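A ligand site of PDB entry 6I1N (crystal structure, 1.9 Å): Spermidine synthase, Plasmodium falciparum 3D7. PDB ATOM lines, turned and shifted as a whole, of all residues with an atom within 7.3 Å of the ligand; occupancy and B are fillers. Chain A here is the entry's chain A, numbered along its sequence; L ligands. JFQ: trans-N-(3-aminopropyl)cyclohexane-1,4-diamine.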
ATOM      1  N   TYR A  71       5.684  -8.396   2.192  1.00  0.00           N
ATOM      2  CA  TYR A  71       5.220  -9.655   2.748  1.00  0.00           C
ATOM      3  C   TYR A  71       4.626  -9.538   4.154  1.00  0.00           C
ATOM      4  O   TYR A  71       3.736 -10.323   4.486  1.00  0.00           O
ATOM      5  CB  TYR A  71       6.363 -10.685   2.758  1.00  0.00           C
ATOM      6  CG  TYR A  71       6.786 -11.044   1.348  1.00  0.00           C
ATOM      7  CD1 TYR A  71       6.036 -11.923   0.577  1.00  0.00           C
ATOM      8  CD2 TYR A  71       7.902 -10.465   0.767  1.00  0.00           C
ATOM      9  CE1 TYR A  71       6.403 -12.243  -0.715  1.00  0.00           C
ATOM     10  CE2 TYR A  71       8.266 -10.764  -0.525  1.00  0.00           C
ATOM     11  CZ  TYR A  71       7.518 -11.664  -1.267  1.00  0.00           C
ATOM     12  OH  TYR A  71       7.893 -11.979  -2.558  1.00  0.00           O
ATOM     13  N   GLN A  72       5.064  -8.584   4.961  1.00  0.00           N
ATOM     14  CA  GLN A  72       4.687  -8.584   6.367  1.00  0.00           C
ATOM     15  C   GLN A  72       4.968  -7.223   6.963  1.00  0.00           C
ATOM     16  O   GLN A  72       5.727  -6.417   6.415  1.00  0.00           O
ATOM     17  CB  GLN A  72       5.434  -9.679   7.141  1.00  0.00           C
ATOM     18  CG  GLN A  72       6.959  -9.563   7.033  1.00  0.00           C
ATOM     19  CD  GLN A  72       7.677 -10.899   7.199  1.00  0.00           C
ATOM     20  OE1 GLN A  72       8.686 -11.170   6.533  1.00  0.00           O
ATOM     21  NE2 GLN A  72       7.176 -11.741   8.099  1.00  0.00           N
ATOM     22  N   LEU A  86      12.743  -8.068  17.535  1.00  0.00           N
ATOM     23  CA  LEU A  86      12.244  -8.060  16.173  1.00  0.00           C
ATOM     24  C   LEU A  86      10.869  -8.712  16.114  1.00  0.00           C
ATOM     25  O   LEU A  86      10.674  -9.846  16.600  1.00  0.00           O
ATOM     26  CB  LEU A  86      13.213  -8.799  15.231  1.00  0.00           C
ATOM     27  CG  LEU A  86      12.684  -9.022  13.801  1.00  0.00           C
ATOM     28  CD1 LEU A  86      12.476  -7.670  13.056  1.00  0.00           C
ATOM     29  CD2 LEU A  86      13.602  -9.939  12.989  1.00  0.00           C
ATOM     30  N   LEU A  88       7.463  -9.577  13.560  1.00  0.00           N
ATOM     31  CA  LEU A  88       6.957  -9.768  12.200  1.00  0.00           C
ATOM     32  C   LEU A  88       5.480 -10.108  12.273  1.00  0.00           C
ATOM     33  O   LEU A  88       5.099 -11.123  12.870  1.00  0.00           O
ATOM     34  CB  LEU A  88       7.741 -10.862  11.465  1.00  0.00           C
ATOM     35  CG  LEU A  88       9.204 -10.542  11.132  1.00  0.00           C
ATOM     36  CD1 LEU A  88       9.853 -11.684  10.351  1.00  0.00           C
ATOM     37  CD2 LEU A  88       9.381  -9.213  10.383  1.00  0.00           C
ATOM     38  N   GLN A  93       9.864 -12.468  16.697  1.00  0.00           N
ATOM     39  CA  GLN A  93      10.824 -13.326  15.996  1.00  0.00           C
ATOM     40  C   GLN A  93      12.045 -13.620  16.821  1.00  0.00           C
ATOM     41  O   GLN A  93      12.613 -14.716  16.728  1.00  0.00           O
ATOM     42  CB  GLN A  93      11.290 -12.660  14.697  1.00  0.00           C
ATOM     43  CG  GLN A  93      10.171 -12.520  13.748  1.00  0.00           C
ATOM     44  CD  GLN A  93       9.587 -13.864  13.399  1.00  0.00           C
ATOM     45  OE1 GLN A  93      10.323 -14.782  12.980  1.00  0.00           O
ATOM     46  NE2 GLN A  93       8.262 -14.007  13.576  1.00  0.00           N
ATOM     47  N   VAL A 123      16.652 -22.198   5.453  1.00  0.00           N
ATOM     48  CA  VAL A 123      15.405 -21.705   4.885  1.00  0.00           C
ATOM     49  C   VAL A 123      14.780 -20.710   5.858  1.00  0.00           C
ATOM     50  O   VAL A 123      14.642 -21.003   7.047  1.00  0.00           O
ATOM     51  CB  VAL A 123      14.455 -22.877   4.569  1.00  0.00           C
ATOM     52  CG1 VAL A 123      13.092 -22.385   4.166  1.00  0.00           C
ATOM     53  CG2 VAL A 123      15.053 -23.760   3.493  1.00  0.00           C
ATOM     54  N   GLY A 124      14.381 -19.531   5.357  1.00  0.00           N
ATOM     55  CA  GLY A 124      13.934 -18.509   6.307  1.00  0.00           C
ATOM     56  C   GLY A 124      15.151 -17.977   7.042  1.00  0.00           C
ATOM     57  O   GLY A 124      16.258 -17.977   6.518  1.00  0.00           O
ATOM     58  N   GLY A 125      14.972 -17.539   8.271  1.00  0.00           N
ATOM     59  CA  GLY A 125      16.204 -17.131   8.978  1.00  0.00           C
ATOM     60  C   GLY A 125      16.869 -15.864   8.470  1.00  0.00           C
ATOM     61  O   GLY A 125      18.102 -15.725   8.570  1.00  0.00           O
ATOM     62  N   GLY A 126      16.079 -14.911   7.965  1.00  0.00           N
ATOM     63  CA  GLY A 126      16.700 -13.686   7.476  1.00  0.00           C
ATOM     64  C   GLY A 126      17.483 -12.956   8.541  1.00  0.00           C
ATOM     65  O   GLY A 126      18.419 -12.236   8.221  1.00  0.00           O
ATOM     66  N   ASP A 127      17.142 -13.156   9.811  1.00  0.00           N
ATOM     67  CA  ASP A 127      17.832 -12.431  10.872  1.00  0.00           C
ATOM     68  C   ASP A 127      19.294 -12.827  11.007  1.00  0.00           C
ATOM     69  O   ASP A 127      20.071 -12.083  11.621  1.00  0.00           O
ATOM     70  CB  ASP A 127      17.109 -12.666  12.186  1.00  0.00           C
ATOM     71  CG  ASP A 127      17.010 -14.155  12.499  1.00  0.00           C
ATOM     72  OD1 ASP A 127      18.070 -14.767  12.791  1.00  0.00           O
ATOM     73  OD2 ASP A 127      15.904 -14.696  12.330  1.00  0.00           O
ATOM     74  N   CYS A 146      17.993 -18.908   2.086  1.00  0.00           N
ATOM     75  CA  CYS A 146      16.877 -18.554   1.235  1.00  0.00           C
ATOM     76  C   CYS A 146      15.829 -17.837   2.094  1.00  0.00           C
ATOM     77  O   CYS A 146      15.239 -18.449   2.988  1.00  0.00           O
ATOM     78  CB  CYS A 146      16.320 -19.816   0.606  1.00  0.00           C
ATOM     79  SG  CYS A 146      15.097 -19.381  -0.591  1.00  0.00           S
ATOM     80  N   GLU A 147      15.596 -16.557   1.809  1.00  0.00           N
ATOM     81  CA  GLU A 147      14.680 -15.749   2.612  1.00  0.00           C
ATOM     82  C   GLU A 147      13.850 -14.892   1.657  1.00  0.00           C
ATOM     83  O   GLU A 147      14.403 -14.195   0.801  1.00  0.00           O
ATOM     84  CB  GLU A 147      15.483 -14.886   3.606  1.00  0.00           C
ATOM     85  CG  GLU A 147      14.724 -13.661   4.131  1.00  0.00           C
ATOM     86  CD  GLU A 147      13.493 -14.054   4.935  1.00  0.00           C
ATOM     87  OE1 GLU A 147      13.654 -14.831   5.912  1.00  0.00           O
ATOM     88  OE2 GLU A 147      12.377 -13.619   4.574  1.00  0.00           O
ATOM     89  N   ILE A 148      12.527 -15.000   1.753  1.00  0.00           N
ATOM     90  CA  ILE A 148      11.664 -14.338   0.789  1.00  0.00           C
ATOM     91  C   ILE A 148      11.625 -12.816   0.950  1.00  0.00           C
ATOM     92  O   ILE A 148      11.304 -12.091  -0.013  1.00  0.00           O
ATOM     93  CB  ILE A 148      10.252 -14.962   0.868  1.00  0.00           C
ATOM     94  CG1 ILE A 148       9.444 -14.677  -0.390  1.00  0.00           C
ATOM     95  CG2 ILE A 148       9.496 -14.488   2.132  1.00  0.00           C
ATOM     96  CD1 ILE A 148       8.074 -15.323  -0.360  1.00  0.00           C
ATOM     97  N   ASP A 149      11.951 -12.293   2.138  1.00  0.00           N
ATOM     98  CA  ASP A 149      11.742 -10.885   2.463  1.00  0.00           C
ATOM     99  C   ASP A 149      13.077 -10.225   2.811  1.00  0.00           C
ATOM    100  O   ASP A 149      13.561 -10.339   3.943  1.00  0.00           O
ATOM    101  CB  ASP A 149      10.733 -10.741   3.611  1.00  0.00           C
ATOM    102  CG  ASP A 149      10.251  -9.286   3.804  1.00  0.00           C
ATOM    103  OD1 ASP A 149      10.908  -8.369   3.250  1.00  0.00           O
ATOM    104  OD2 ASP A 149       9.230  -9.070   4.509  1.00  0.00           O
ATOM    105  N   GLU A 150      13.661  -9.498   1.846  1.00  0.00           N
ATOM    106  CA  GLU A 150      14.968  -8.897   2.093  1.00  0.00           C
ATOM    107  C   GLU A 150      14.950  -7.813   3.171  1.00  0.00           C
ATOM    108  O   GLU A 150      16.004  -7.548   3.772  1.00  0.00           O
ATOM    109  CB  GLU A 150      15.540  -8.328   0.789  1.00  0.00           C
ATOM    110  CG  GLU A 150      14.701  -7.281   0.131  1.00  0.00           C
ATOM    111  CD  GLU A 150      15.324  -6.836  -1.199  1.00  0.00           C
ATOM    112  OE1 GLU A 150      16.541  -6.530  -1.212  1.00  0.00           O
ATOM    113  OE2 GLU A 150      14.602  -6.823  -2.220  1.00  0.00           O
ATOM    114  N   VAL A 152      13.700  -8.107   6.135  1.00  0.00           N
ATOM    115  CA  VAL A 152      14.162  -8.834   7.324  1.00  0.00           C
ATOM    116  C   VAL A 152      15.685  -8.811   7.407  1.00  0.00           C
ATOM    117  O   VAL A 152      16.274  -8.355   8.397  1.00  0.00           O
ATOM    118  CB  VAL A 152      13.606 -10.267   7.318  1.00  0.00           C
ATOM    119  CG1 VAL A 152      14.181 -11.086   8.502  1.00  0.00           C
ATOM    120  CG2 VAL A 152      12.107 -10.244   7.355  1.00  0.00           C
ATOM    121  N   PHE A 175      19.785 -15.724  -1.200  1.00  0.00           N
ATOM    122  CA  PHE A 175      18.782 -15.849  -2.251  1.00  0.00           C
ATOM    123  C   PHE A 175      17.480 -15.241  -1.762  1.00  0.00           C
ATOM    124  O   PHE A 175      16.850 -15.781  -0.830  1.00  0.00           O
ATOM    125  CB  PHE A 175      18.606 -17.299  -2.651  1.00  0.00           C
ATOM    126  CG  PHE A 175      19.871 -17.922  -3.162  1.00  0.00           C
ATOM    127  CD1 PHE A 175      20.787 -18.514  -2.286  1.00  0.00           C
ATOM    128  CD2 PHE A 175      20.184 -17.868  -4.521  1.00  0.00           C
ATOM    129  CE1 PHE A 175      21.959 -19.078  -2.751  1.00  0.00           C
ATOM    130  CE2 PHE A 175      21.371 -18.434  -5.006  1.00  0.00           C
ATOM    131  CZ  PHE A 175      22.262 -19.044  -4.121  1.00  0.00           C
ATOM    132  N   GLU A 177      13.983 -15.155  -2.268  1.00  0.00           N
ATOM    133  CA  GLU A 177      13.270 -16.119  -3.087  1.00  0.00           C
ATOM    134  C   GLU A 177      12.386 -16.974  -2.183  1.00  0.00           C
ATOM    135  O   GLU A 177      12.711 -17.212  -1.026  1.00  0.00           O
ATOM    136  CB  GLU A 177      14.305 -16.976  -3.855  1.00  0.00           C
ATOM    137  CG  GLU A 177      13.788 -18.132  -4.653  1.00  0.00           C
ATOM    138  CD  GLU A 177      14.831 -18.662  -5.635  1.00  0.00           C
ATOM    139  OE1 GLU A 177      16.043 -18.518  -5.356  1.00  0.00           O
ATOM    140  OE2 GLU A 177      14.424 -19.199  -6.686  1.00  0.00           O
ATOM    141  N   ASP A 178      11.251 -17.405  -2.735  1.00  0.00           N
ATOM    142  CA  ASP A 178      10.381 -18.371  -2.100  1.00  0.00           C
ATOM    143  C   ASP A 178      11.099 -19.707  -1.954  1.00  0.00           C
ATOM    144  O   ASP A 178      11.748 -20.182  -2.892  1.00  0.00           O
ATOM    145  CB  ASP A 178       9.130 -18.517  -2.961  1.00  0.00           C
ATOM    146  CG  ASP A 178       8.369 -19.761  -2.637  1.00  0.00           C
ATOM    147  OD1 ASP A 178       7.690 -19.768  -1.594  1.00  0.00           O
ATOM    148  OD2 ASP A 178       8.446 -20.719  -3.433  1.00  0.00           O
ATOM    149  N   ALA A 179      10.980 -20.355  -0.790  1.00  0.00           N
ATOM    150  CA  ALA A 179      11.774 -21.561  -0.553  1.00  0.00           C
ATOM    151  C   ALA A 179      11.355 -22.713  -1.457  1.00  0.00           C
ATOM    152  O   ALA A 179      12.203 -23.550  -1.813  1.00  0.00           O
ATOM    153  CB  ALA A 179      11.686 -21.991   0.910  1.00  0.00           C
ATOM    154  N   SER A 180      10.079 -22.795  -1.840  1.00  0.00           N
ATOM    155  CA  SER A 180       9.673 -23.877  -2.745  1.00  0.00           C
ATOM    156  C   SER A 180      10.303 -23.698  -4.122  1.00  0.00           C
ATOM    157  O   SER A 180      10.721 -24.678  -4.744  1.00  0.00           O
ATOM    158  CB  SER A 180       8.156 -23.924  -2.887  1.00  0.00           C
ATOM    159  OG  SER A 180       7.597 -24.741  -1.880  1.00  0.00           O
ATOM    160  N   LYS A 181      10.365 -22.463  -4.614  1.00  0.00           N
ATOM    161  CA  LYS A 181      11.064 -22.230  -5.869  1.00  0.00           C
ATOM    162  C   LYS A 181      12.562 -22.504  -5.744  1.00  0.00           C
ATOM    163  O   LYS A 181      13.168 -23.129  -6.632  1.00  0.00           O
ATOM    164  CB  LYS A 181      10.807 -20.803  -6.357  1.00  0.00           C
ATOM    165  CG  LYS A 181      11.369 -20.562  -7.738  1.00  0.00           C
ATOM    166  CD  LYS A 181      11.346 -19.089  -8.127  1.00  0.00           C
ATOM    167  CE  LYS A 181      12.236 -18.818  -9.344  1.00  0.00           C
ATOM    168  NZ  LYS A 181      12.046 -17.431  -9.879  1.00  0.00           N
ATOM    169  N   ASP A 196      14.230 -22.522   9.310  1.00  0.00           N
ATOM    170  CA  ASP A 196      14.025 -21.570  10.381  1.00  0.00           C
ATOM    171  C   ASP A 196      12.830 -20.676  10.030  1.00  0.00           C
ATOM    172  O   ASP A 196      12.975 -19.497   9.742  1.00  0.00           O
ATOM    173  CB  ASP A 196      15.287 -20.769  10.644  1.00  0.00           C
ATOM    174  CG  ASP A 196      15.087 -19.667  11.684  1.00  0.00           C
ATOM    175  OD1 ASP A 196      14.065 -19.709  12.402  1.00  0.00           O
ATOM    176  OD2 ASP A 196      15.934 -18.773  11.788  1.00  0.00           O
ATOM    177  N   SER A 197      11.648 -21.275  10.048  1.00  0.00           N
ATOM    178  CA  SER A 197      10.438 -20.630   9.570  1.00  0.00           C
ATOM    179  C   SER A 197       9.213 -21.349  10.108  1.00  0.00           C
ATOM    180  O   SER A 197       9.224 -22.585  10.223  1.00  0.00           O
ATOM    181  CB  SER A 197      10.386 -20.607   8.046  1.00  0.00           C
ATOM    182  OG  SER A 197       9.039 -20.620   7.600  1.00  0.00           O
ATOM    183  N   SER A 198       8.153 -20.590  10.396  1.00  0.00           N
ATOM    184  CA  SER A 198       6.883 -21.172  10.860  1.00  0.00           C
ATOM    185  C   SER A 198       6.186 -21.918   9.719  1.00  0.00           C
ATOM    186  O   SER A 198       5.909 -21.336   8.660  1.00  0.00           O
ATOM    187  CB  SER A 198       5.941 -20.088  11.409  1.00  0.00           C
ATOM    188  OG  SER A 198       6.545 -19.326  12.436  1.00  0.00           O
ATOM    189  N   PHE A 212       6.442 -30.156   0.508  1.00  0.00           N
ATOM    190  CA  PHE A 212       7.631 -29.413   0.909  1.00  0.00           C
ATOM    191  C   PHE A 212       8.696 -30.341   1.455  1.00  0.00           C
ATOM    192  O   PHE A 212       9.899 -30.141   1.192  1.00  0.00           O
ATOM    193  CB  PHE A 212       7.257 -28.360   1.952  1.00  0.00           C
ATOM    194  CG  PHE A 212       8.399 -27.501   2.390  1.00  0.00           C
ATOM    195  CD1 PHE A 212       8.908 -26.517   1.548  1.00  0.00           C
ATOM    196  CD2 PHE A 212       8.983 -27.675   3.637  1.00  0.00           C
ATOM    197  CE1 PHE A 212       9.962 -25.721   1.943  1.00  0.00           C
ATOM    198  CE2 PHE A 212      10.036 -26.880   4.042  1.00  0.00           C
ATOM    199  CZ  PHE A 212      10.523 -25.899   3.190  1.00  0.00           C
HETATM  200  C1  JFQ L   1      10.503 -14.140   7.925  1.00  0.00           C
HETATM  201  N1  JFQ L   1      10.496 -13.614   6.557  1.00  0.00           N
HETATM  202  C2  JFQ L   1      11.485 -15.285   8.220  1.00  0.00           C
HETATM  203  N2  JFQ L   1      11.307 -16.283   6.042  1.00  0.00           N
HETATM  204  C3  JFQ L   1      11.105 -16.550   7.468  1.00  0.00           C
HETATM  205  N3  JFQ L   1       9.541 -19.507   1.642  1.00  0.00           N
HETATM  206  C4  JFQ L   1      10.940 -17.386   5.139  1.00  0.00           C
HETATM  207  C5  JFQ L   1      11.408 -16.943   3.752  1.00  0.00           C
HETATM  208  C6  JFQ L   1      11.169 -18.011   2.683  1.00  0.00           C
HETATM  209  C7  JFQ L   1       9.696 -18.438   2.637  1.00  0.00           C
HETATM  210  C8  JFQ L   1       9.163 -18.842   4.041  1.00  0.00           C
HETATM  211  C9  JFQ L   1       9.444 -17.781   5.111  1.00  0.00           C
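The side-chain carboxylate (OE2) of Glu 147 lies within salt-bridge range of a nitrogen (N1) of the ligand (2.7 Å). N3 of the ligand is in salt-bridge range of OD1 of Asp 178, at 3.7 Å. The side-chain amide oxygen of Gln 72 lies within hydrogen-bond range of a nitrogen (N1) of the ligand. N of Ala 179 lies close to N3 of the ligand, 3.0 Å away.
N of Ser 180 lies within hydrogen-bond range of OD2 of Asp 178, at 3.1 Å. OE1 of Gln 72 sits close to OD2 of Asp 149, 3.0 Å away. The backbone NH (N) of Glu 177 is in hydrogen-bond range of the backbone carbonyl oxygen (O) of Glu 147 (3.2 Å). The backbone carbonyl oxygen (O) of Phe 175 lies within hydrogen-bond range of the backbone NH (N) of Glu 147. OE2 of Glu 147 is in hydrogen-bond range of N of Asp 149 (2.8 Å). The side-chain carboxylate (OD2) of Asp 178 is in hydrogen-bond range of the backbone NH (N) of Lys 181 (2.8 Å). N of Gly 126 is in hydrogen-bond range of OE1 of Glu 147. N of Gly 124 is in hydrogen-bond range of O of Cys 146.
Residues that only touch the ligand: Leu 88 (3.5 Å), Gly 124 (3.4 Å), Ile 148 (3.0 Å), Val 152 (3.8 Å) and Ser 197 (3.8 Å). Within 4 Å of the ligand: Gln 72, Leu 88, Gly 124, Glu 147, Ile 148, Val 152, Asp 178, Ala 179 and Ser 197. The nearest printed residue that does not touch the ligand is Gly 125 (4.1 Å).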
